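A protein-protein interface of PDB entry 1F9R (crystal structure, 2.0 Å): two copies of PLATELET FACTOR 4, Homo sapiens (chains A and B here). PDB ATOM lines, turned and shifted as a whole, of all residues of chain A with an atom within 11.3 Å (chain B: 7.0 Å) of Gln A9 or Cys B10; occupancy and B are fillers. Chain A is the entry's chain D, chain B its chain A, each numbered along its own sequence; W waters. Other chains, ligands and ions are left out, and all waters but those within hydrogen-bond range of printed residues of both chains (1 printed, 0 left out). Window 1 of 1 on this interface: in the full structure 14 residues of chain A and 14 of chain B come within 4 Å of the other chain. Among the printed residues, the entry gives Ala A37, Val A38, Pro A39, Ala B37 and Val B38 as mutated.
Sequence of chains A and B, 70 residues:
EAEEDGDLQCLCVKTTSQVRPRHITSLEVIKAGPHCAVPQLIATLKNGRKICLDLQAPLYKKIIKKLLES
Of the printed residues of chain B, Leu A8 touches Leu B11 and Val B13.
Of the printed residues of chain B, Cys A10 touches Gln B9.
Printed residues of chain B within 4 Å of Val A13: Gln B9.
Of the printed residues of chain B, Lys A50 touches Leu B8.
Printed residues of chain B within 4 Å of Cys A52: Leu B8 (3.4 Å).
Cys B10 touches one residue of chain A.
Cys B12 touches one residue of chain A.
Val B13 touches three residues of chain A.
No residue of chain A comes within 4 Å of Cys B36.
Ala B37 touches none of the printed residues of chain A.
No residue of chain A comes within 4 Å of Val B38.
The nearest residue of chain B that does not touch Gln A9 is Cys B12 (4.5 Å).
The nearest residue of chain A that does not touch Cys B10 is Cys A10 (4.4 Å).
The nearest printed residue of chain B that does not touch Leu A8 is Cys B12 (4.7 Å).
Of the 12 printed residues of chain B, 6 touch a printed residue of chain A.
Printed residues of chain B that touch a printed residue of chain A: Leu B8, Gln B9, Cys B10, Leu B11, Cys B12 and Val B13.
Hydrophobic or aromatic side chains of chain B that line the printed part of chain A: Leu B8, Leu B11 and Val B13.
Of the 23 printed residues of chain A, 8 touch a printed residue of chain B.
Hydrophobic or aromatic side chains of chain A within 4 Å of the printed part of chain B: Leu A8, Leu A11 and Val A13.
The backbone carbonyl oxygen (O) of Cys A10 is in hydrogen-bond range of the side-chain amide nitrogen (NE2) of Gln B9, 2.8 Å away.
The backbone NH (N) of Gln B9 sits at hydrogen-bond distance from the backbone carbonyl oxygen (O) of Leu A11, 2.9 Å away.
The side-chain amide nitrogen (NE2) of Gln A9 lies within hydrogen-bond range of the backbone carbonyl oxygen (O) of Cys B10 (2.9 Å).
The backbone carbonyl oxygen of Leu B11 is in hydrogen-bond range of the backbone NH of Gln A9, at 2.9 Å.
The backbone NH (N) of Val B13 is in hydrogen-bond range of the backbone carbonyl oxygen (O) of Asp A7 (2.7 Å).
The backbone carbonyl oxygen of His B35 lies within hydrogen-bond range of the backbone NH of Cys B10 (3.0 Å).
The side-chain sulfur (SG) of Cys B10 is disulfide-bonded to the side-chain sulfur (SG) of Cys B36, at 2.0 Å.
N of Leu B11 lies within hydrogen-bond range of OE1 of Gln B40 (2.8 Å).
The backbone NH (N) of Cys B12 lies within hydrogen-bond range of the side-chain amide oxygen (OE1) of Gln B40.
The backbone NH (N) of Cys A10 lies within hydrogen-bond range of the backbone carbonyl oxygen (O) of His A35 (3.4 Å).
OE1 of Gln A40 sits at hydrogen-bond distance from N of Leu A11.
Among the printed residues, pairs that only touch across the chains: Leu A8 with Leu B11, Leu A11 with Leu B8, Cys A52 with Leu B8, Gln A9 with Val B13, Asp A7 with Cys B12, Val A13 with Gln B9, Leu A11 with Leu B11, Gln A9 with Gln B9, Leu A8 with Val B13, Lys A50 with Leu B8 and Asp A7 with Leu B11.
Leu A8 touches Leu B11, and with the chains exchanged Leu A11 touches Leu B8.
Gln A9 touches its own counterpart, Gln B9.
Gln A9 touches Cys B10, and with the chains exchanged Cys A10 touches Gln B9.
Gln A9 touches Val B13, and with the chains exchanged Val A13 touches Gln B9.
Of the 16 pairs that touch across the chains among the printed residues, 10 have their exchanged pair printed and touching as well.
Water W1 bridges the side-chain amide oxygen of Gln B9 (2.8 Å) and the side-chain amide oxygen of Gln A9 (3.1 Å).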
ATOM      1  N   GLY A   6     -36.635  -3.149  -0.454  1.00  0.00           N
ATOM      2  CA  GLY A   6     -37.306  -3.311  -1.790  1.00  0.00           C
ATOM      3  C   GLY A   6     -37.389  -4.763  -2.219  1.00  0.00           C
ATOM      4  O   GLY A   6     -36.875  -5.645  -1.530  1.00  0.00           O
ATOM      5  N   ASP A   7     -38.023  -5.013  -3.360  1.00  0.00           N
ATOM      6  CA  ASP A   7     -38.169  -6.367  -3.886  1.00  0.00           C
ATOM      7  C   ASP A   7     -36.948  -6.867  -4.657  1.00  0.00           C
ATOM      8  O   ASP A   7     -36.702  -8.069  -4.728  1.00  0.00           O
ATOM      9  CB  ASP A   7     -39.389  -6.451  -4.810  1.00  0.00           C
ATOM     10  CG  ASP A   7     -40.673  -6.755  -4.067  1.00  0.00           C
ATOM     11  OD1 ASP A   7     -41.716  -6.899  -4.742  1.00  0.00           O
ATOM     12  OD2 ASP A   7     -40.642  -6.853  -2.822  1.00  0.00           O
ATOM     13  N   LEU A   8     -36.182  -5.947  -5.229  1.00  0.00           N
ATOM     14  CA  LEU A   8     -35.016  -6.326  -6.016  1.00  0.00           C
ATOM     15  C   LEU A   8     -33.671  -6.091  -5.333  1.00  0.00           C
ATOM     16  O   LEU A   8     -33.506  -5.153  -4.556  1.00  0.00           O
ATOM     17  CB  LEU A   8     -35.041  -5.586  -7.362  1.00  0.00           C
ATOM     18  CG  LEU A   8     -36.262  -5.818  -8.264  1.00  0.00           C
ATOM     19  CD1 LEU A   8     -37.519  -5.298  -7.597  1.00  0.00           C
ATOM     20  CD2 LEU A   8     -36.058  -5.101  -9.589  1.00  0.00           C
ATOM     21  N   GLN A   9     -32.717  -6.970  -5.631  1.00  0.00           N
ATOM     22  CA  GLN A   9     -31.360  -6.873  -5.099  1.00  0.00           C
ATOM     23  C   GLN A   9     -30.436  -6.701  -6.310  1.00  0.00           C
ATOM     24  O   GLN A   9     -30.910  -6.627  -7.443  1.00  0.00           O
ATOM     25  CB  GLN A   9     -30.994  -8.152  -4.342  1.00  0.00           C
ATOM     26  CG  GLN A   9     -30.626  -9.327  -5.241  1.00  0.00           C
ATOM     27  CD  GLN A   9     -30.476 -10.613  -4.460  1.00  0.00           C
ATOM     28  OE1 GLN A   9     -29.987 -10.603  -3.334  1.00  0.00           O
ATOM     29  NE2 GLN A   9     -30.889 -11.730  -5.054  1.00  0.00           N
ATOM     30  N   CYS A  10     -29.128  -6.635  -6.085  1.00  0.00           N
ATOM     31  CA  CYS A  10     -28.208  -6.486  -7.205  1.00  0.00           C
ATOM     32  C   CYS A  10     -28.116  -7.785  -7.997  1.00  0.00           C
ATOM     33  O   CYS A  10     -27.904  -8.863  -7.435  1.00  0.00           O
ATOM     34  CB  CYS A  10     -26.798  -6.114  -6.741  1.00  0.00           C
ATOM     35  SG  CYS A  10     -26.602  -4.563  -5.822  1.00  0.00           S
ATOM     36  N   LEU A  11     -28.278  -7.657  -9.306  1.00  0.00           N
ATOM     37  CA  LEU A  11     -28.208  -8.767 -10.243  1.00  0.00           C
ATOM     38  C   LEU A  11     -26.819  -9.418 -10.224  1.00  0.00           C
ATOM     39  O   LEU A  11     -26.688 -10.646 -10.321  1.00  0.00           O
ATOM     40  CB  LEU A  11     -28.501  -8.241 -11.643  1.00  0.00           C
ATOM     41  CG  LEU A  11     -28.471  -9.226 -12.804  1.00  0.00           C
ATOM     42  CD1 LEU A  11     -29.558 -10.281 -12.614  1.00  0.00           C
ATOM     43  CD2 LEU A  11     -28.681  -8.453 -14.114  1.00  0.00           C
ATOM     44  N   CYS A  12     -25.793  -8.580 -10.098  1.00  0.00           N
ATOM     45  CA  CYS A  12     -24.403  -9.026 -10.079  1.00  0.00           C
ATOM     46  C   CYS A  12     -23.911  -9.374  -8.684  1.00  0.00           C
ATOM     47  O   CYS A  12     -23.765  -8.502  -7.834  1.00  0.00           O
ATOM     48  CB  CYS A  12     -23.496  -7.938 -10.648  1.00  0.00           C
ATOM     49  SG  CYS A  12     -23.819  -7.454 -12.369  1.00  0.00           S
ATOM     50  N   VAL A  13     -23.630 -10.651  -8.456  1.00  0.00           N
ATOM     51  CA  VAL A  13     -23.148 -11.089  -7.156  1.00  0.00           C
ATOM     52  C   VAL A  13     -21.626 -11.079  -7.153  1.00  0.00           C
ATOM     53  O   VAL A  13     -21.000 -11.238  -6.116  1.00  0.00           O
ATOM     54  CB  VAL A  13     -23.664 -12.504  -6.819  1.00  0.00           C
ATOM     55  CG1 VAL A  13     -23.022 -13.528  -7.745  1.00  0.00           C
ATOM     56  CG2 VAL A  13     -23.384 -12.829  -5.359  1.00  0.00           C
ATOM     57  N   LYS A  14     -21.038 -10.902  -8.329  1.00  0.00           N
ATOM     58  CA  LYS A  14     -19.585 -10.821  -8.466  1.00  0.00           C
ATOM     59  C   LYS A  14     -19.252 -10.358  -9.878  1.00  0.00           C
ATOM     60  O   LYS A  14     -20.142 -10.256 -10.722  1.00  0.00           O
ATOM     61  CB  LYS A  14     -18.914 -12.171  -8.169  1.00  0.00           C
ATOM     62  CG  LYS A  14     -19.180 -13.281  -9.162  1.00  0.00           C
ATOM     63  CD  LYS A  14     -18.545 -14.582  -8.658  1.00  0.00           C
ATOM     64  CE  LYS A  14     -18.675 -15.735  -9.655  1.00  0.00           C
ATOM     65  NZ  LYS A  14     -17.888 -15.506 -10.904  1.00  0.00           N
ATOM     66  N   ILE A  30     -26.759  -0.638 -16.125  1.00  0.00           N
ATOM     67  CA  ILE A  30     -27.856  -0.388 -15.193  1.00  0.00           C
ATOM     68  C   ILE A  30     -27.426   0.616 -14.124  1.00  0.00           C
ATOM     69  O   ILE A  30     -26.547   0.335 -13.306  1.00  0.00           O
ATOM     70  CB  ILE A  30     -28.284  -1.704 -14.492  1.00  0.00           C
ATOM     71  CG1 ILE A  30     -28.607  -2.776 -15.540  1.00  0.00           C
ATOM     72  CG2 ILE A  30     -29.540  -1.471 -13.642  1.00  0.00           C
ATOM     73  CD1 ILE A  30     -28.806  -4.174 -14.961  1.00  0.00           C
ATOM     74  N   LYS A  31     -28.047   1.789 -14.107  1.00  0.00           N
ATOM     75  CA  LYS A  31     -27.649   2.768 -13.115  1.00  0.00           C
ATOM     76  C   LYS A  31     -28.089   2.362 -11.720  1.00  0.00           C
ATOM     77  O   LYS A  31     -29.028   1.581 -11.550  1.00  0.00           O
ATOM     78  CB  LYS A  31     -28.204   4.147 -13.451  1.00  0.00           C
ATOM     79  CG  LYS A  31     -29.678   4.328 -13.203  1.00  0.00           C
ATOM     80  CD  LYS A  31     -30.083   5.796 -13.419  1.00  0.00           C
ATOM     81  CE  LYS A  31     -29.179   6.734 -12.616  1.00  0.00           C
ATOM     82  NZ  LYS A  31     -29.649   8.146 -12.573  1.00  0.00           N
ATOM     83  N   ALA A  32     -27.373   2.872 -10.724  1.00  0.00           N
ATOM     84  CA  ALA A  32     -27.678   2.601  -9.325  1.00  0.00           C
ATOM     85  C   ALA A  32     -29.099   3.069  -9.006  1.00  0.00           C
ATOM     86  O   ALA A  32     -29.604   4.004  -9.612  1.00  0.00           O
ATOM     87  CB  ALA A  32     -26.676   3.322  -8.435  1.00  0.00           C
ATOM     88  N   GLY A  33     -29.742   2.412  -8.051  1.00  0.00           N
ATOM     89  CA  GLY A  33     -31.098   2.775  -7.686  1.00  0.00           C
ATOM     90  C   GLY A  33     -31.502   2.016  -6.441  1.00  0.00           C
ATOM     91  O   GLY A  33     -30.632   1.513  -5.735  1.00  0.00           O
ATOM     92  N   PRO A  34     -32.807   1.913  -6.140  1.00  0.00           N
ATOM     93  CA  PRO A  34     -33.257   1.189  -4.943  1.00  0.00           C
ATOM     94  C   PRO A  34     -32.867  -0.283  -5.005  1.00  0.00           C
ATOM     95  O   PRO A  34     -32.723  -0.951  -3.981  1.00  0.00           O
ATOM     96  CB  PRO A  34     -34.773   1.372  -4.971  1.00  0.00           C
ATOM     97  CG  PRO A  34     -34.948   2.678  -5.697  1.00  0.00           C
ATOM     98  CD  PRO A  34     -33.945   2.557  -6.819  1.00  0.00           C
ATOM     99  N   HIS A  35     -32.697  -0.772  -6.225  1.00  0.00           N
ATOM    100  CA  HIS A  35     -32.336  -2.157  -6.488  1.00  0.00           C
ATOM    101  C   HIS A  35     -30.876  -2.475  -6.174  1.00  0.00           C
ATOM    102  O   HIS A  35     -30.557  -3.585  -5.743  1.00  0.00           O
ATOM    103  CB  HIS A  35     -32.588  -2.473  -7.966  1.00  0.00           C
ATOM    104  CG  HIS A  35     -31.718  -1.689  -8.900  1.00  0.00           C
ATOM    105  ND1 HIS A  35     -31.978  -0.375  -9.235  1.00  0.00           N
ATOM    106  CD2 HIS A  35     -30.555  -2.011  -9.520  1.00  0.00           C
ATOM    107  CE1 HIS A  35     -31.014   0.077 -10.015  1.00  0.00           C
ATOM    108  NE2 HIS A  35     -30.137  -0.895 -10.203  1.00  0.00           N
ATOM    109  N   CYS A  36     -30.002  -1.496  -6.397  1.00  0.00           N
ATOM    110  CA  CYS A  36     -28.572  -1.672  -6.197  1.00  0.00           C
ATOM    111  C   CYS A  36     -27.876  -0.307  -6.003  1.00  0.00           C
ATOM    112  O   CYS A  36     -28.101   0.636  -6.776  1.00  0.00           O
ATOM    113  CB  CYS A  36     -28.009  -2.417  -7.421  1.00  0.00           C
ATOM    114  SG  CYS A  36     -26.340  -3.094  -7.212  1.00  0.00           S
ATOM    115  N   ALA A  37     -27.020  -0.206  -4.985  1.00  0.00           N
ATOM    116  CA  ALA A  37     -26.334   1.048  -4.691  1.00  0.00           C
ATOM    117  C   ALA A  37     -25.235   1.428  -5.665  1.00  0.00           C
ATOM    118  O   ALA A  37     -24.706   2.541  -5.599  1.00  0.00           O
ATOM    119  CB  ALA A  37     -25.777   1.027  -3.271  1.00  0.00           C
ATOM    120  N   VAL A  38     -24.883   0.518  -6.565  1.00  0.00           N
ATOM    121  CA  VAL A  38     -23.850   0.811  -7.547  1.00  0.00           C
ATOM    122  C   VAL A  38     -24.306   0.489  -8.963  1.00  0.00           C
ATOM    123  O   VAL A  38     -25.288  -0.225  -9.168  1.00  0.00           O
ATOM    124  CB  VAL A  38     -22.557   0.005  -7.290  1.00  0.00           C
ATOM    125  CG1 VAL A  38     -21.844   0.523  -6.054  1.00  0.00           C
ATOM    126  CG2 VAL A  38     -22.885  -1.468  -7.149  1.00  0.00           C
ATOM    127  N   PRO A  39     -23.613   1.052  -9.965  1.00  0.00           N
ATOM    128  CA  PRO A  39     -23.980   0.765 -11.352  1.00  0.00           C
ATOM    129  C   PRO A  39     -23.561  -0.692 -11.598  1.00  0.00           C
ATOM    130  O   PRO A  39     -22.803  -1.268 -10.804  1.00  0.00           O
ATOM    131  CB  PRO A  39     -23.116   1.742 -12.148  1.00  0.00           C
ATOM    132  CG  PRO A  39     -22.899   2.891 -11.175  1.00  0.00           C
ATOM    133  CD  PRO A  39     -22.641   2.163  -9.890  1.00  0.00           C
ATOM    134  N   GLN A  40     -24.060  -1.296 -12.673  1.00  0.00           N
ATOM    135  CA  GLN A  40     -23.695  -2.671 -13.004  1.00  0.00           C
ATOM    136  C   GLN A  40     -23.483  -2.754 -14.505  1.00  0.00           C
ATOM    137  O   GLN A  40     -24.233  -2.163 -15.274  1.00  0.00           O
ATOM    138  CB  GLN A  40     -24.796  -3.652 -12.573  1.00  0.00           C
ATOM    139  CG  GLN A  40     -25.034  -3.689 -11.070  1.00  0.00           C
ATOM    140  CD  GLN A  40     -26.309  -4.433 -10.698  1.00  0.00           C
ATOM    141  OE1 GLN A  40     -26.289  -5.629 -10.405  1.00  0.00           O
ATOM    142  NE2 GLN A  40     -27.433  -3.720 -10.730  1.00  0.00           N
ATOM    143  N   ILE A  42     -23.418  -5.322 -17.477  1.00  0.00           N
ATOM    144  CA  ILE A  42     -23.781  -6.671 -17.894  1.00  0.00           C
ATOM    145  C   ILE A  42     -23.399  -6.918 -19.339  1.00  0.00           C
ATOM    146  O   ILE A  42     -23.991  -6.340 -20.255  1.00  0.00           O
ATOM    147  CB  ILE A  42     -25.311  -6.933 -17.760  1.00  0.00           C
ATOM    148  CG1 ILE A  42     -25.845  -6.370 -16.436  1.00  0.00           C
ATOM    149  CG2 ILE A  42     -25.593  -8.432 -17.864  1.00  0.00           C
ATOM    150  CD1 ILE A  42     -25.235  -6.976 -15.207  1.00  0.00           C
ATOM    151  N   LYS A  50     -23.644 -14.429 -19.569  1.00  0.00           N
ATOM    152  CA  LYS A  50     -23.666 -13.053 -19.107  1.00  0.00           C
ATOM    153  C   LYS A  50     -22.731 -12.910 -17.920  1.00  0.00           C
ATOM    154  O   LYS A  50     -22.795 -13.688 -16.973  1.00  0.00           O
ATOM    155  CB  LYS A  50     -25.091 -12.645 -18.724  1.00  0.00           C
ATOM    156  CG  LYS A  50     -26.057 -12.658 -19.907  1.00  0.00           C
ATOM    157  CD  LYS A  50     -27.502 -12.370 -19.498  1.00  0.00           C
ATOM    158  CE  LYS A  50     -27.688 -10.955 -18.980  1.00  0.00           C
ATOM    159  NZ  LYS A  50     -29.124 -10.619 -18.724  1.00  0.00           N
ATOM    160  N   CYS A  52     -20.518  -9.852 -15.357  1.00  0.00           N
ATOM    161  CA  CYS A  52     -20.556  -8.474 -14.906  1.00  0.00           C
ATOM    162  C   CYS A  52     -19.132  -7.943 -14.883  1.00  0.00           C
ATOM    163  O   CYS A  52     -18.197  -8.659 -14.524  1.00  0.00           O
ATOM    164  CB  CYS A  52     -21.184  -8.388 -13.518  1.00  0.00           C
ATOM    165  SG  CYS A  52     -22.921  -8.928 -13.440  1.00  0.00           S
ATOM    166  N   LEU B   8     -24.234 -13.840 -12.294  1.00  0.00           N
ATOM    167  CA  LEU B   8     -25.560 -13.326 -11.927  1.00  0.00           C
ATOM    168  C   LEU B   8     -26.356 -14.155 -10.924  1.00  0.00           C
ATOM    169  O   LEU B   8     -26.130 -15.356 -10.763  1.00  0.00           O
ATOM    170  CB  LEU B   8     -26.417 -13.133 -13.183  1.00  0.00           C
ATOM    171  CG  LEU B   8     -25.909 -12.141 -14.233  1.00  0.00           C
ATOM    172  CD1 LEU B   8     -26.917 -12.032 -15.367  1.00  0.00           C
ATOM    173  CD2 LEU B   8     -25.702 -10.794 -13.591  1.00  0.00           C
ATOM    174  N   GLN B   9     -27.298 -13.490 -10.262  1.00  0.00           N
ATOM    175  CA  GLN B   9     -28.173 -14.112  -9.277  1.00  0.00           C
ATOM    176  C   GLN B   9     -29.584 -13.577  -9.512  1.00  0.00           C
ATOM    177  O   GLN B   9     -29.773 -12.690 -10.339  1.00  0.00           O
ATOM    178  CB  GLN B   9     -27.706 -13.781  -7.852  1.00  0.00           C
ATOM    179  CG  GLN B   9     -27.906 -12.330  -7.388  1.00  0.00           C
ATOM    180  CD  GLN B   9     -27.260 -12.078  -6.040  1.00  0.00           C
ATOM    181  OE1 GLN B   9     -27.180 -12.983  -5.213  1.00  0.00           O
ATOM    182  NE2 GLN B   9     -26.806 -10.845  -5.805  1.00  0.00           N
ATOM    183  N   CYS B  10     -30.567 -14.115  -8.795  1.00  0.00           N
ATOM    184  CA  CYS B  10     -31.942 -13.665  -8.963  1.00  0.00           C
ATOM    185  C   CYS B  10     -32.015 -12.171  -8.703  1.00  0.00           C
ATOM    186  O   CYS B  10     -31.274 -11.630  -7.887  1.00  0.00           O
ATOM    187  CB  CYS B  10     -32.901 -14.388  -7.999  1.00  0.00           C
ATOM    188  SG  CYS B  10     -32.958 -16.206  -8.127  1.00  0.00           S
ATOM    189  N   LEU B  11     -32.905 -11.501  -9.412  1.00  0.00           N
ATOM    190  CA  LEU B  11     -33.079 -10.073  -9.239  1.00  0.00           C
ATOM    191  C   LEU B  11     -34.073  -9.888  -8.098  1.00  0.00           C
ATOM    192  O   LEU B  11     -33.946  -8.992  -7.263  1.00  0.00           O
ATOM    193  CB  LEU B  11     -33.644  -9.483 -10.520  1.00  0.00           C
ATOM    194  CG  LEU B  11     -33.535  -7.980 -10.744  1.00  0.00           C
ATOM    195  CD1 LEU B  11     -32.065  -7.581 -10.756  1.00  0.00           C
ATOM    196  CD2 LEU B  11     -34.209  -7.615 -12.078  1.00  0.00           C
ATOM    197  N   CYS B  12     -35.050 -10.782  -8.065  1.00  0.00           N
ATOM    198  CA  CYS B  12     -36.116 -10.756  -7.083  1.00  0.00           C
ATOM    199  C   CYS B  12     -35.746 -11.399  -5.768  1.00  0.00           C
ATOM    200  O   CYS B  12     -35.225 -12.513  -5.732  1.00  0.00           O
ATOM    201  CB  CYS B  12     -37.345 -11.452  -7.650  1.00  0.00           C
ATOM    202  SG  CYS B  12     -38.058 -10.596  -9.086  1.00  0.00           S
ATOM    203  N   VAL B  13     -36.048 -10.685  -4.688  1.00  0.00           N
ATOM    204  CA  VAL B  13     -35.766 -11.133  -3.331  1.00  0.00           C
ATOM    205  C   VAL B  13     -37.043 -11.698  -2.729  1.00  0.00           C
ATOM    206  O   VAL B  13     -37.025 -12.707  -2.033  1.00  0.00           O
ATOM    207  CB  VAL B  13     -35.304  -9.953  -2.459  1.00  0.00           C
ATOM    208  CG1 VAL B  13     -34.801 -10.450  -1.119  1.00  0.00           C
ATOM    209  CG2 VAL B  13     -34.238  -9.162  -3.189  1.00  0.00           C
ATOM    210  N   PRO B  34     -29.260 -20.223 -15.229  1.00  0.00           N
ATOM    211  CA  PRO B  34     -28.076 -20.122 -14.359  1.00  0.00           C
ATOM    212  C   PRO B  34     -28.217 -19.021 -13.299  1.00  0.00           C
ATOM    213  O   PRO B  34     -27.898 -19.213 -12.129  1.00  0.00           O
ATOM    214  CB  PRO B  34     -26.944 -19.808 -15.349  1.00  0.00           C
ATOM    215  CG  PRO B  34     -27.421 -20.393 -16.640  1.00  0.00           C
ATOM    216  CD  PRO B  34     -28.888 -20.030 -16.644  1.00  0.00           C
ATOM    217  N   HIS B  35     -28.693 -17.868 -13.747  1.00  0.00           N
ATOM    218  CA  HIS B  35     -28.899 -16.685 -12.920  1.00  0.00           C
ATOM    219  C   HIS B  35     -29.914 -16.888 -11.801  1.00  0.00           C
ATOM    220  O   HIS B  35     -29.768 -16.349 -10.702  1.00  0.00           O
ATOM    221  CB  HIS B  35     -29.388 -15.555 -13.824  1.00  0.00           C
ATOM    222  CG  HIS B  35     -30.630 -15.905 -14.583  1.00  0.00           C
ATOM    223  ND1 HIS B  35     -31.896 -15.686 -14.082  1.00  0.00           N
ATOM    224  CD2 HIS B  35     -30.798 -16.555 -15.761  1.00  0.00           C
ATOM    225  CE1 HIS B  35     -32.790 -16.190 -14.915  1.00  0.00           C
ATOM    226  NE2 HIS B  35     -32.151 -16.724 -15.941  1.00  0.00           N
ATOM    227  N   CYS B  36     -30.948 -17.664 -12.096  1.00  0.00           N
ATOM    228  CA  CYS B  36     -32.013 -17.902 -11.138  1.00  0.00           C
ATOM    229  C   CYS B  36     -32.766 -19.168 -11.530  1.00  0.00           C
ATOM    230  O   CYS B  36     -33.089 -19.362 -12.701  1.00  0.00           O
ATOM    231  CB  CYS B  36     -32.947 -16.685 -11.132  1.00  0.00           C
ATOM    232  SG  CYS B  36     -34.120 -16.600  -9.753  1.00  0.00           S
ATOM    233  N   ALA B  37     -33.032 -20.029 -10.549  1.00  0.00           N
ATOM    234  CA  ALA B  37     -33.725 -21.296 -10.789  1.00  0.00           C
ATOM    235  C   ALA B  37     -35.231 -21.159 -10.980  1.00  0.00           C
ATOM    236  O   ALA B  37     -35.898 -22.123 -11.358  1.00  0.00           O
ATOM    237  CB  ALA B  37     -33.431 -22.282  -9.657  1.00  0.00           C
ATOM    238  N   VAL B  38     -35.760 -19.966 -10.721  1.00  0.00           N
ATOM    239  CA  VAL B  38     -37.185 -19.710 -10.896  1.00  0.00           C
ATOM    240  C   VAL B  38     -37.459 -18.523 -11.828  1.00  0.00           C
ATOM    241  O   VAL B  38     -36.635 -17.623 -11.966  1.00  0.00           O
ATOM    242  CB  VAL B  38     -37.878 -19.396  -9.548  1.00  0.00           C
ATOM    243  CG1 VAL B  38     -37.817 -20.604  -8.613  1.00  0.00           C
ATOM    244  CG2 VAL B  38     -37.229 -18.185  -8.907  1.00  0.00           C
ATOM    245  N   GLN B  40     -39.041 -15.002 -13.141  1.00  0.00           N
ATOM    246  CA  GLN B  40     -39.227 -13.756 -12.429  1.00  0.00           C
ATOM    247  C   GLN B  40     -40.192 -12.828 -13.161  1.00  0.00           C
ATOM    248  O   GLN B  40     -40.205 -12.765 -14.388  1.00  0.00           O
ATOM    249  CB  GLN B  40     -37.880 -13.086 -12.229  1.00  0.00           C
ATOM    250  CG  GLN B  40     -36.867 -13.998 -11.563  1.00  0.00           C
ATOM    251  CD  GLN B  40     -35.490 -13.355 -11.454  1.00  0.00           C
ATOM    252  OE1 GLN B  40     -35.249 -12.516 -10.576  1.00  0.00           O
ATOM    253  NE2 GLN B  40     -34.586 -13.732 -12.360  1.00  0.00           N
HETATM  254  O   HOH W   1     -27.570 -12.346  -2.466  1.00  0.00           O
